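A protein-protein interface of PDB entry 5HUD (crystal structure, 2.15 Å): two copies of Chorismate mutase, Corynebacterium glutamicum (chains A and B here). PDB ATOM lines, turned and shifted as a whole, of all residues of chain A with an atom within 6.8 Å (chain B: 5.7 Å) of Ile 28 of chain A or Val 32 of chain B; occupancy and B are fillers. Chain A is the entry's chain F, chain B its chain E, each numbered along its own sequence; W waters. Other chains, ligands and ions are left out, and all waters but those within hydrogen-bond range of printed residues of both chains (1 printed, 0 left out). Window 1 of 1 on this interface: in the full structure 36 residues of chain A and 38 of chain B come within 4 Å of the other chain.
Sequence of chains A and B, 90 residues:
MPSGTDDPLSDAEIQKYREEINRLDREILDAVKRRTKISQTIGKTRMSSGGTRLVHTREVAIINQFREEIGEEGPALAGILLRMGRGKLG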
ATOM      1  N   ILE A  21      -4.107  15.954 -32.486  1.00  0.00           N
ATOM      2  CA  ILE A  21      -4.942  16.779 -31.581  1.00  0.00           C
ATOM      3  C   ILE A  21      -4.767  16.317 -30.144  1.00  0.00           C
ATOM      4  O   ILE A  21      -4.552  17.130 -29.243  1.00  0.00           O
ATOM      5  CB  ILE A  21      -6.458  16.800 -31.987  1.00  0.00           C
ATOM      6  CG1 ILE A  21      -6.650  17.741 -33.186  1.00  0.00           C
ATOM      7  CG2 ILE A  21      -7.371  17.267 -30.837  1.00  0.00           C
ATOM      8  CD1 ILE A  21      -7.962  17.586 -33.904  1.00  0.00           C
ATOM      9  N   ARG A  23      -2.269  14.772 -28.712  1.00  0.00           N
ATOM     10  CA  ARG A  23      -0.953  15.204 -28.216  1.00  0.00           C
ATOM     11  C   ARG A  23      -0.911  16.707 -27.878  1.00  0.00           C
ATOM     12  O   ARG A  23      -0.304  17.129 -26.882  1.00  0.00           O
ATOM     13  CB  ARG A  23       0.141  14.860 -29.243  1.00  0.00           C
ATOM     14  CG  ARG A  23       1.567  14.739 -28.686  1.00  0.00           C
ATOM     15  CD  ARG A  23       2.644  14.585 -29.772  1.00  0.00           C
ATOM     16  NE  ARG A  23       2.098  14.272 -31.108  1.00  0.00           N
ATOM     17  CZ  ARG A  23       1.705  13.066 -31.553  1.00  0.00           C
ATOM     18  NH1 ARG A  23       1.215  12.949 -32.794  1.00  0.00           N
ATOM     19  NH2 ARG A  23       1.785  11.973 -30.783  1.00  0.00           N
ATOM     20  N   LEU A  24      -1.546  17.500 -28.729  1.00  0.00           N
ATOM     21  CA  LEU A  24      -1.729  18.920 -28.464  1.00  0.00           C
ATOM     22  C   LEU A  24      -2.630  19.202 -27.254  1.00  0.00           C
ATOM     23  O   LEU A  24      -2.402  20.157 -26.521  1.00  0.00           O
ATOM     24  CB  LEU A  24      -2.293  19.617 -29.713  1.00  0.00           C
ATOM     25  CG  LEU A  24      -1.264  19.761 -30.837  1.00  0.00           C
ATOM     26  CD1 LEU A  24      -1.951  20.085 -32.152  1.00  0.00           C
ATOM     27  CD2 LEU A  24      -0.209  20.817 -30.473  1.00  0.00           C
ATOM     28  N   ASP A  25      -3.662  18.387 -27.065  1.00  0.00           N
ATOM     29  CA  ASP A  25      -4.508  18.513 -25.881  1.00  0.00           C
ATOM     30  C   ASP A  25      -3.740  18.215 -24.591  1.00  0.00           C
ATOM     31  O   ASP A  25      -3.854  18.993 -23.635  1.00  0.00           O
ATOM     32  CB  ASP A  25      -5.812  17.738 -26.032  1.00  0.00           C
ATOM     33  CG  ASP A  25      -6.759  18.393 -27.068  1.00  0.00           C
ATOM     34  OD1 ASP A  25      -6.495  19.568 -27.480  1.00  0.00           O
ATOM     35  OD2 ASP A  25      -7.764  17.741 -27.486  1.00  0.00           O
ATOM     36  N   ARG A  26      -2.936  17.150 -24.579  1.00  0.00           N
ATOM     37  CA  ARG A  26      -1.997  16.902 -23.478  1.00  0.00           C
ATOM     38  C   ARG A  26      -1.067  18.091 -23.190  1.00  0.00           C
ATOM     39  O   ARG A  26      -0.828  18.421 -22.022  1.00  0.00           O
ATOM     40  CB  ARG A  26      -1.134  15.676 -23.767  1.00  0.00           C
ATOM     41  CG  ARG A  26      -1.906  14.400 -24.039  1.00  0.00           C
ATOM     42  CD  ARG A  26      -0.942  13.244 -24.255  1.00  0.00           C
ATOM     43  NE  ARG A  26      -1.539  12.151 -25.018  1.00  0.00           N
ATOM     44  CZ  ARG A  26      -1.091  11.750 -26.199  1.00  0.00           C
ATOM     45  NH1 ARG A  26      -1.676  10.748 -26.832  1.00  0.00           N
ATOM     46  NH2 ARG A  26      -0.039  12.346 -26.727  1.00  0.00           N
ATOM     47  N   GLU A  27      -0.559  18.730 -24.248  1.00  0.00           N
ATOM     48  CA  GLU A  27       0.342  19.875 -24.103  1.00  0.00           C
ATOM     49  C   GLU A  27      -0.332  21.122 -23.482  1.00  0.00           C
ATOM     50  O   GLU A  27       0.201  21.724 -22.538  1.00  0.00           O
ATOM     51  CB  GLU A  27       0.999  20.250 -25.444  1.00  0.00           C
ATOM     52  CG  GLU A  27       1.993  21.415 -25.318  1.00  0.00           C
ATOM     53  CD  GLU A  27       2.717  21.773 -26.620  1.00  0.00           C
ATOM     54  OE1 GLU A  27       2.408  21.167 -27.703  1.00  0.00           O
ATOM     55  OE2 GLU A  27       3.608  22.675 -26.542  1.00  0.00           O
ATOM     56  N   ILE A  28      -1.478  21.511 -24.048  1.00  0.00           N
ATOM     57  CA  ILE A  28      -2.329  22.574 -23.508  1.00  0.00           C
ATOM     58  C   ILE A  28      -2.617  22.284 -22.035  1.00  0.00           C
ATOM     59  O   ILE A  28      -2.298  23.093 -21.178  1.00  0.00           O
ATOM     60  CB  ILE A  28      -3.640  22.681 -24.329  1.00  0.00           C
ATOM     61  CG1 ILE A  28      -3.324  23.250 -25.716  1.00  0.00           C
ATOM     62  CG2 ILE A  28      -4.694  23.575 -23.665  1.00  0.00           C
ATOM     63  CD1 ILE A  28      -4.410  23.003 -26.743  1.00  0.00           C
ATOM     64  N   LEU A  29      -3.119  21.082 -21.754  1.00  0.00           N
ATOM     65  CA  LEU A  29      -3.473  20.645 -20.386  1.00  0.00           C
ATOM     66  C   LEU A  29      -2.306  20.564 -19.409  1.00  0.00           C
ATOM     67  O   LEU A  29      -2.459  20.930 -18.248  1.00  0.00           O
ATOM     68  CB  LEU A  29      -4.185  19.288 -20.417  1.00  0.00           C
ATOM     69  CG  LEU A  29      -5.564  19.273 -21.042  1.00  0.00           C
ATOM     70  CD1 LEU A  29      -5.906  17.850 -21.430  1.00  0.00           C
ATOM     71  CD2 LEU A  29      -6.623  19.824 -20.087  1.00  0.00           C
ATOM     72  N   ASP A  30      -1.161  20.058 -19.861  1.00  0.00           N
ATOM     73  CA  ASP A  30       0.059  20.069 -19.048  1.00  0.00           C
ATOM     74  C   ASP A  30       0.452  21.506 -18.746  1.00  0.00           C
ATOM     75  O   ASP A  30       0.704  21.812 -17.606  1.00  0.00           O
ATOM     76  CB  ASP A  30       1.219  19.308 -19.727  1.00  0.00           C
ATOM     77  CG  ASP A  30       2.566  19.452 -18.975  1.00  0.00           C
ATOM     78  OD1 ASP A  30       3.548  20.052 -19.524  1.00  0.00           O
ATOM     79  OD2 ASP A  30       2.661  18.945 -17.836  1.00  0.00           O
ATOM     80  N   ALA A  31       0.465  22.380 -19.747  1.00  0.00           N
ATOM     81  CA  ALA A  31       0.861  23.796 -19.551  1.00  0.00           C
ATOM     82  C   ALA A  31      -0.122  24.607 -18.709  1.00  0.00           C
ATOM     83  O   ALA A  31       0.310  25.493 -17.957  1.00  0.00           O
ATOM     84  CB  ALA A  31       1.092  24.503 -20.887  1.00  0.00           C
ATOM     85  N   VAL A  32      -1.426  24.324 -18.851  1.00  0.00           N
ATOM     86  CA  VAL A  32      -2.458  24.979 -18.007  1.00  0.00           C
ATOM     87  C   VAL A  32      -2.235  24.656 -16.542  1.00  0.00           C
ATOM     88  O   VAL A  32      -2.270  25.542 -15.709  1.00  0.00           O
ATOM     89  CB  VAL A  32      -3.912  24.624 -18.451  1.00  0.00           C
ATOM     90  CG1 VAL A  32      -4.962  24.971 -17.376  1.00  0.00           C
ATOM     91  CG2 VAL A  32      -4.232  25.347 -19.746  1.00  0.00           C
ATOM     92  N   LYS A  33      -1.995  23.391 -16.240  1.00  0.00           N
ATOM     93  CA  LYS A  33      -1.636  22.968 -14.856  1.00  0.00           C
ATOM     94  C   LYS A  33      -0.442  23.722 -14.281  1.00  0.00           C
ATOM     95  O   LYS A  33      -0.523  24.259 -13.187  1.00  0.00           O
ATOM     96  CB  LYS A  33      -1.350  21.459 -14.784  1.00  0.00           C
ATOM     97  CG  LYS A  33      -2.598  20.605 -14.692  1.00  0.00           C
ATOM     98  CD  LYS A  33      -2.378  19.214 -15.274  1.00  0.00           C
ATOM     99  CE  LYS A  33      -3.463  18.272 -14.825  1.00  0.00           C
ATOM    100  NZ  LYS A  33      -3.564  17.124 -15.757  1.00  0.00           N
ATOM    101  N   ILE A  70      -6.013  35.396 -30.558  1.00  0.00           N
ATOM    102  CA  ILE A  70      -6.931  34.421 -31.189  1.00  0.00           C
ATOM    103  C   ILE A  70      -8.336  34.913 -31.548  1.00  0.00           C
ATOM    104  O   ILE A  70      -9.111  34.148 -32.093  1.00  0.00           O
ATOM    105  CB  ILE A  70      -7.053  33.107 -30.371  1.00  0.00           C
ATOM    106  CG1 ILE A  70      -7.523  33.353 -28.925  1.00  0.00           C
ATOM    107  CG2 ILE A  70      -5.726  32.360 -30.372  1.00  0.00           C
ATOM    108  CD1 ILE A  70      -7.997  32.071 -28.267  1.00  0.00           C
ATOM    109  N   LEU A  77     -10.869  32.151 -23.106  1.00  0.00           N
ATOM    110  CA  LEU A  77      -9.723  31.298 -22.833  1.00  0.00           C
ATOM    111  C   LEU A  77      -8.939  31.852 -21.634  1.00  0.00           C
ATOM    112  O   LEU A  77      -8.565  31.100 -20.731  1.00  0.00           O
ATOM    113  CB  LEU A  77      -8.837  31.173 -24.071  1.00  0.00           C
ATOM    114  CG  LEU A  77      -7.567  30.366 -23.858  1.00  0.00           C
ATOM    115  CD1 LEU A  77      -7.888  28.948 -23.439  1.00  0.00           C
ATOM    116  CD2 LEU A  77      -6.713  30.418 -25.119  1.00  0.00           C
ATOM    117  N   LEU A  81      -8.028  30.627 -17.478  1.00  0.00           N
ATOM    118  CA  LEU A  81      -6.707  30.586 -16.869  1.00  0.00           C
ATOM    119  C   LEU A  81      -6.672  31.465 -15.663  1.00  0.00           C
ATOM    120  O   LEU A  81      -5.978  31.175 -14.685  1.00  0.00           O
ATOM    121  CB  LEU A  81      -5.612  31.010 -17.859  1.00  0.00           C
ATOM    122  CG  LEU A  81      -5.543  30.133 -19.137  1.00  0.00           C
ATOM    123  CD1 LEU A  81      -4.405  30.640 -19.982  1.00  0.00           C
ATOM    124  CD2 LEU A  81      -5.475  28.610 -18.944  1.00  0.00           C
ATOM    125  N   GLU B  27       3.166  29.451 -25.246  1.00  0.00           N
ATOM    126  CA  GLU B  27       3.047  28.019 -25.506  1.00  0.00           C
ATOM    127  C   GLU B  27       1.590  27.523 -25.669  1.00  0.00           C
ATOM    128  O   GLU B  27       1.296  26.790 -26.597  1.00  0.00           O
ATOM    129  CB  GLU B  27       3.757  27.222 -24.396  1.00  0.00           C
ATOM    130  CG  GLU B  27       3.450  25.732 -24.427  1.00  0.00           C
ATOM    131  CD  GLU B  27       4.457  24.870 -23.691  1.00  0.00           C
ATOM    132  OE1 GLU B  27       5.288  25.428 -22.923  1.00  0.00           O
ATOM    133  OE2 GLU B  27       4.402  23.635 -23.912  1.00  0.00           O
ATOM    134  N   ILE B  28       0.704  27.895 -24.741  1.00  0.00           N
ATOM    135  CA  ILE B  28      -0.735  27.504 -24.824  1.00  0.00           C
ATOM    136  C   ILE B  28      -1.371  28.106 -26.098  1.00  0.00           C
ATOM    137  O   ILE B  28      -2.006  27.411 -26.851  1.00  0.00           O
ATOM    138  CB  ILE B  28      -1.557  27.922 -23.558  1.00  0.00           C
ATOM    139  CG1 ILE B  28      -1.059  27.255 -22.272  1.00  0.00           C
ATOM    140  CG2 ILE B  28      -3.024  27.559 -23.703  1.00  0.00           C
ATOM    141  CD1 ILE B  28      -1.307  28.085 -21.018  1.00  0.00           C
ATOM    142  N   LEU B  29      -1.169  29.395 -26.330  1.00  0.00           N
ATOM    143  CA  LEU B  29      -1.669  30.059 -27.520  1.00  0.00           C
ATOM    144  C   LEU B  29      -1.199  29.354 -28.808  1.00  0.00           C
ATOM    145  O   LEU B  29      -2.031  28.954 -29.655  1.00  0.00           O
ATOM    146  CB  LEU B  29      -1.250  31.538 -27.507  1.00  0.00           C
ATOM    147  CG  LEU B  29      -2.012  32.459 -26.535  1.00  0.00           C
ATOM    148  CD1 LEU B  29      -1.409  33.866 -26.459  1.00  0.00           C
ATOM    149  CD2 LEU B  29      -3.504  32.545 -26.916  1.00  0.00           C
ATOM    150  N   ASP B  30       0.119  29.118 -28.908  1.00  0.00           N
ATOM    151  CA  ASP B  30       0.702  28.453 -30.069  1.00  0.00           C
ATOM    152  C   ASP B  30       0.171  27.026 -30.227  1.00  0.00           C
ATOM    153  O   ASP B  30      -0.064  26.570 -31.339  1.00  0.00           O
ATOM    154  CB  ASP B  30       2.246  28.483 -30.034  1.00  0.00           C
ATOM    155  CG  ASP B  30       2.831  29.903 -30.239  1.00  0.00           C
ATOM    156  OD1 ASP B  30       3.889  30.218 -29.644  1.00  0.00           O
ATOM    157  OD2 ASP B  30       2.235  30.721 -30.988  1.00  0.00           O
ATOM    158  N   ALA B  31      -0.054  26.324 -29.129  1.00  0.00           N
ATOM    159  CA  ALA B  31      -0.643  24.997 -29.208  1.00  0.00           C
ATOM    160  C   ALA B  31      -2.070  25.073 -29.761  1.00  0.00           C
ATOM    161  O   ALA B  31      -2.412  24.361 -30.704  1.00  0.00           O
ATOM    162  CB  ALA B  31      -0.638  24.337 -27.849  1.00  0.00           C
ATOM    163  N   VAL B  32      -2.874  25.972 -29.183  1.00  0.00           N
ATOM    164  CA  VAL B  32      -4.268  26.166 -29.583  1.00  0.00           C
ATOM    165  C   VAL B  32      -4.362  26.458 -31.091  1.00  0.00           C
ATOM    166  O   VAL B  32      -5.195  25.865 -31.791  1.00  0.00           O
ATOM    167  CB  VAL B  32      -4.949  27.288 -28.754  1.00  0.00           C
ATOM    168  CG1 VAL B  32      -6.308  27.693 -29.330  1.00  0.00           C
ATOM    169  CG2 VAL B  32      -5.112  26.834 -27.307  1.00  0.00           C
ATOM    170  N   LYS B  33      -3.495  27.336 -31.585  1.00  0.00           N
ATOM    171  CA  LYS B  33      -3.508  27.701 -33.017  1.00  0.00           C
ATOM    172  C   LYS B  33      -3.245  26.490 -33.952  1.00  0.00           C
ATOM    173  O   LYS B  33      -3.956  26.308 -34.971  1.00  0.00           O
ATOM    174  CB  LYS B  33      -2.542  28.864 -33.316  1.00  0.00           C
ATOM    175  CG  LYS B  33      -2.893  30.214 -32.671  1.00  0.00           C
ATOM    176  CD  LYS B  33      -1.729  31.183 -32.790  1.00  0.00           C
ATOM    177  CE  LYS B  33      -2.139  32.588 -32.437  1.00  0.00           C
ATOM    178  NZ  LYS B  33      -0.986  33.531 -32.239  1.00  0.00           N
ATOM    179  N   ARG B  34      -2.291  25.634 -33.599  1.00  0.00           N
ATOM    180  CA  ARG B  34      -2.033  24.478 -34.466  1.00  0.00           C
ATOM    181  C   ARG B  34      -3.138  23.417 -34.337  1.00  0.00           C
ATOM    182  O   ARG B  34      -3.595  22.874 -35.339  1.00  0.00           O
ATOM    183  CB  ARG B  34      -0.624  23.894 -34.303  1.00  0.00           C
ATOM    184  CG  ARG B  34      -0.020  23.479 -35.656  1.00  0.00           C
ATOM    185  CD  ARG B  34       1.412  22.995 -35.517  1.00  0.00           C
ATOM    186  NE  ARG B  34       1.453  21.740 -34.766  1.00  0.00           N
ATOM    187  CZ  ARG B  34       2.422  21.347 -33.928  1.00  0.00           C
ATOM    188  NH1 ARG B  34       3.507  22.102 -33.688  1.00  0.00           N
ATOM    189  NH2 ARG B  34       2.297  20.172 -33.299  1.00  0.00           N
ATOM    190  N   ARG B  35      -3.591  23.155 -33.113  1.00  0.00           N
ATOM    191  CA  ARG B  35      -4.811  22.357 -32.887  1.00  0.00           C
ATOM    192  C   ARG B  35      -5.976  22.763 -33.818  1.00  0.00           C
ATOM    193  O   ARG B  35      -6.578  21.931 -34.464  1.00  0.00           O
ATOM    194  CB  ARG B  35      -5.257  22.457 -31.424  1.00  0.00           C
ATOM    195  CG  ARG B  35      -6.196  21.334 -31.011  1.00  0.00           C
ATOM    196  CD  ARG B  35      -7.098  21.734 -29.859  1.00  0.00           C
ATOM    197  NE  ARG B  35      -8.031  20.647 -29.544  1.00  0.00           N
ATOM    198  CZ  ARG B  35      -9.179  20.405 -30.183  1.00  0.00           C
ATOM    199  NH1 ARG B  35      -9.916  19.364 -29.811  1.00  0.00           N
ATOM    200  NH2 ARG B  35      -9.588  21.167 -31.213  1.00  0.00           N
ATOM    201  N   THR B  36      -6.254  24.054 -33.882  1.00  0.00           N
ATOM    202  CA  THR B  36      -7.380  24.593 -34.628  1.00  0.00           C
ATOM    203  C   THR B  36      -7.205  24.441 -36.138  1.00  0.00           C
ATOM    204  O   THR B  36      -8.187  24.135 -36.823  1.00  0.00           O
ATOM    205  CB  THR B  36      -7.618  26.063 -34.206  1.00  0.00           C
ATOM    206  OG1 THR B  36      -7.951  26.076 -32.813  1.00  0.00           O
ATOM    207  CG2 THR B  36      -8.720  26.751 -34.991  1.00  0.00           C
ATOM    208  N   LYS B  37      -5.989  24.642 -36.670  1.00  0.00           N
ATOM    209  CA  LYS B  37      -5.677  24.224 -38.063  1.00  0.00           C
ATOM    210  C   LYS B  37      -6.063  22.773 -38.290  1.00  0.00           C
ATOM    211  O   LYS B  37      -6.762  22.457 -39.236  1.00  0.00           O
ATOM    212  CB  LYS B  37      -4.192  24.331 -38.409  1.00  0.00           C
ATOM    213  CG  LYS B  37      -3.706  25.649 -38.967  1.00  0.00           C
ATOM    214  CD  LYS B  37      -2.262  25.457 -39.457  1.00  0.00           C
ATOM    215  CE  LYS B  37      -1.365  26.662 -39.194  1.00  0.00           C
ATOM    216  NZ  LYS B  37      -1.583  27.720 -40.224  1.00  0.00           N
ATOM    217  N   PHE B  66     -11.061  16.317 -20.603  1.00  0.00           N
ATOM    218  CA  PHE B  66     -10.653  17.616 -20.053  1.00  0.00           C
ATOM    219  C   PHE B  66     -11.105  17.804 -18.615  1.00  0.00           C
ATOM    220  O   PHE B  66     -10.325  18.264 -17.776  1.00  0.00           O
ATOM    221  CB  PHE B  66     -11.168  18.761 -20.937  1.00  0.00           C
ATOM    222  CG  PHE B  66     -10.237  19.107 -22.058  1.00  0.00           C
ATOM    223  CD1 PHE B  66      -9.799  18.130 -22.942  1.00  0.00           C
ATOM    224  CD2 PHE B  66      -9.758  20.411 -22.213  1.00  0.00           C
ATOM    225  CE1 PHE B  66      -8.912  18.438 -23.953  1.00  0.00           C
ATOM    226  CE2 PHE B  66      -8.880  20.717 -23.220  1.00  0.00           C
ATOM    227  CZ  PHE B  66      -8.454  19.730 -24.093  1.00  0.00           C
ATOM    228  N   LEU B  77     -12.905  24.872 -21.293  1.00  0.00           N
ATOM    229  CA  LEU B  77     -11.697  24.857 -22.119  1.00  0.00           C
ATOM    230  C   LEU B  77     -11.887  24.028 -23.398  1.00  0.00           C
ATOM    231  O   LEU B  77     -11.560  24.506 -24.501  1.00  0.00           O
ATOM    232  CB  LEU B  77     -10.486  24.317 -21.353  1.00  0.00           C
ATOM    233  CG  LEU B  77      -9.151  24.402 -22.124  1.00  0.00           C
ATOM    234  CD1 LEU B  77      -8.854  25.821 -22.634  1.00  0.00           C
ATOM    235  CD2 LEU B  77      -8.020  23.878 -21.237  1.00  0.00           C
ATOM    236  N   LEU B  81     -11.986  25.184 -27.573  1.00  0.00           N
ATOM    237  CA  LEU B  81     -11.207  24.541 -28.626  1.00  0.00           C
ATOM    238  C   LEU B  81     -12.139  23.982 -29.704  1.00  0.00           C
ATOM    239  O   LEU B  81     -11.844  24.116 -30.891  1.00  0.00           O
ATOM    240  CB  LEU B  81     -10.271  23.455 -28.064  1.00  0.00           C
ATOM    241  CG  LEU B  81      -9.200  23.934 -27.087  1.00  0.00           C
ATOM    242  CD1 LEU B  81      -8.365  22.760 -26.645  1.00  0.00           C
ATOM    243  CD2 LEU B  81      -8.312  25.023 -27.643  1.00  0.00           C
ATOM    244  N   MET B  84     -13.465  26.787 -31.737  1.00  0.00           N
ATOM    245  CA  MET B  84     -12.344  27.199 -32.602  1.00  0.00           C
ATOM    246  C   MET B  84     -12.153  26.225 -33.765  1.00  0.00           C
ATOM    247  O   MET B  84     -12.005  26.643 -34.906  1.00  0.00           O
ATOM    248  CB  MET B  84     -11.052  27.335 -31.792  1.00  0.00           C
ATOM    249  CG  MET B  84     -11.076  28.565 -30.910  1.00  0.00           C
ATOM    250  SD  MET B  84      -9.539  28.942 -30.073  1.00  0.00           S
ATOM    251  CE  MET B  84      -8.673  29.901 -31.324  1.00  0.00           C
HETATM  252  O   HOH W   1       3.101  25.118 -27.732  1.00  0.00           O
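OE2 of Glu 27 of chain A sits close to OE2 of Glu 27 of chain B (2.9 Å). The guanidinium group (NE) of Arg 35 of chain B is in salt-bridge range of the side-chain carboxylate (OD1) of Asp 25 of chain A, 2.8 Å away.
O of Val 32 of chain B is in hydrogen-bond range of OG1 of Thr 36 of chain B, 2.9 Å away.
Arg 35 of chain B touches Ile 21 of chain A (NH1 to CG2, 3.5 Å). Leu 24 of chain A touches Arg 34 of chain B (CD2 to NH2, 3.8 Å). CD1 of Leu 24 of chain A touches N of Arg 35 of chain B (3.6 Å). Asp 25 of chain A touches Phe 66 of chain B (CG to CZ, 3.7 Å). CG1 of Ile 28 of chain A touches CB of Ala 31 of chain B, at 3.6 Å. CD1 of Ile 28 of chain A touches CD1 of Leu 81 of chain B, at 3.96 Å. Leu 29 of chain A touches Phe 66 of chain B (CD2 to CD2, 3.8 Å). Ile 28 of chain B touches Ala 31 of chain A (CG1 to CB, 3.8 Å). CB of Ile 70 of chain A touches CE of Met 84 of chain B, 3.7 Å away. Leu 77 of chain B touches Leu 77 of chain A (CD1 to CD1, 3.4 Å).
Ile 28 of chain A touches just these residues of chain B: Ala 31 (3.6 Å), Val 32 (3.9 Å) and Leu 81 (3.96 Å). Printed residues of chain A within 4 Å of Val 32 of chain B: Ile 28. Printed residues of chain B within 4 Å of Glu 27 of chain A: Glu 27. Of the printed residues of chain A, Leu 81 of chain B touches Asp 25 (3.8 Å) and Ile 28 (3.96 Å). Printed residues of chain A within 4 Å of Phe 66 of chain B: Asp 25 (3.7 Å) and Leu 29 (3.8 Å). Asp 30 of chain A touches none of the printed residues of chain B. Lys 37 of chain B touches none of the printed residues of chain A. The nearest residue of chain A that does not touch Val 32 of chain B is Leu 77 of chain A (4.5 Å).
Of the 15 printed residues of chain A, 9 touch a printed residue of chain B. Printed residues of chain A that touch a printed residue of chain B: Ile 21, Leu 24, Asp 25, Glu 27, Ile 28, Leu 29, Ala 31, Ile 70 and Leu 77. Of the 15 printed residues of chain B, 10 touch a printed residue of chain A. Printed residues of chain B that touch a printed residue of chain A: Glu 27, Ile 28, Ala 31, Val 32, Arg 34, Arg 35, Phe 66, Leu 77, Leu 81 and Met 84. Hydrophobic or aromatic side chains of chain B that line the printed part of chain A: Ile 28, Ala 31, Val 32, Phe 66, Leu 77, Leu 81 and Met 84. Among the printed residues, 14 pairs touch across the chains.
Ile 28 of chain A touches Ala 31 of chain B, and with the chains exchanged Ala 31 of chain A touches Ile 28 of chain B. Ile 28 of chain A touches Val 32 of chain B, but with the chains exchanged Val 32 of chain A does not touch Ile 28 of chain B (4.2 Å). Ile 28 of chain A touches Leu 81 of chain B, but with the chains exchanged Leu 81 of chain A does not touch Ile 28 of chain B (4.1 Å). Leu 77 of chain A touches its own counterpart, Leu 77 of chain B. Positions printed for both chains: 27, 28, 29, 30, 31, 32, 33, 77 and 81. Of the 14 pairs that touch across the chains among the printed residues, 4 have their exchanged pair printed and touching as well.
Water W1 lies within hydrogen-bond range of the backbone carbonyl oxygen of Glu 27 of chain B (2.7 Å) and the side-chain carboxylate of Glu 27 of chain A (2.8 Å).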
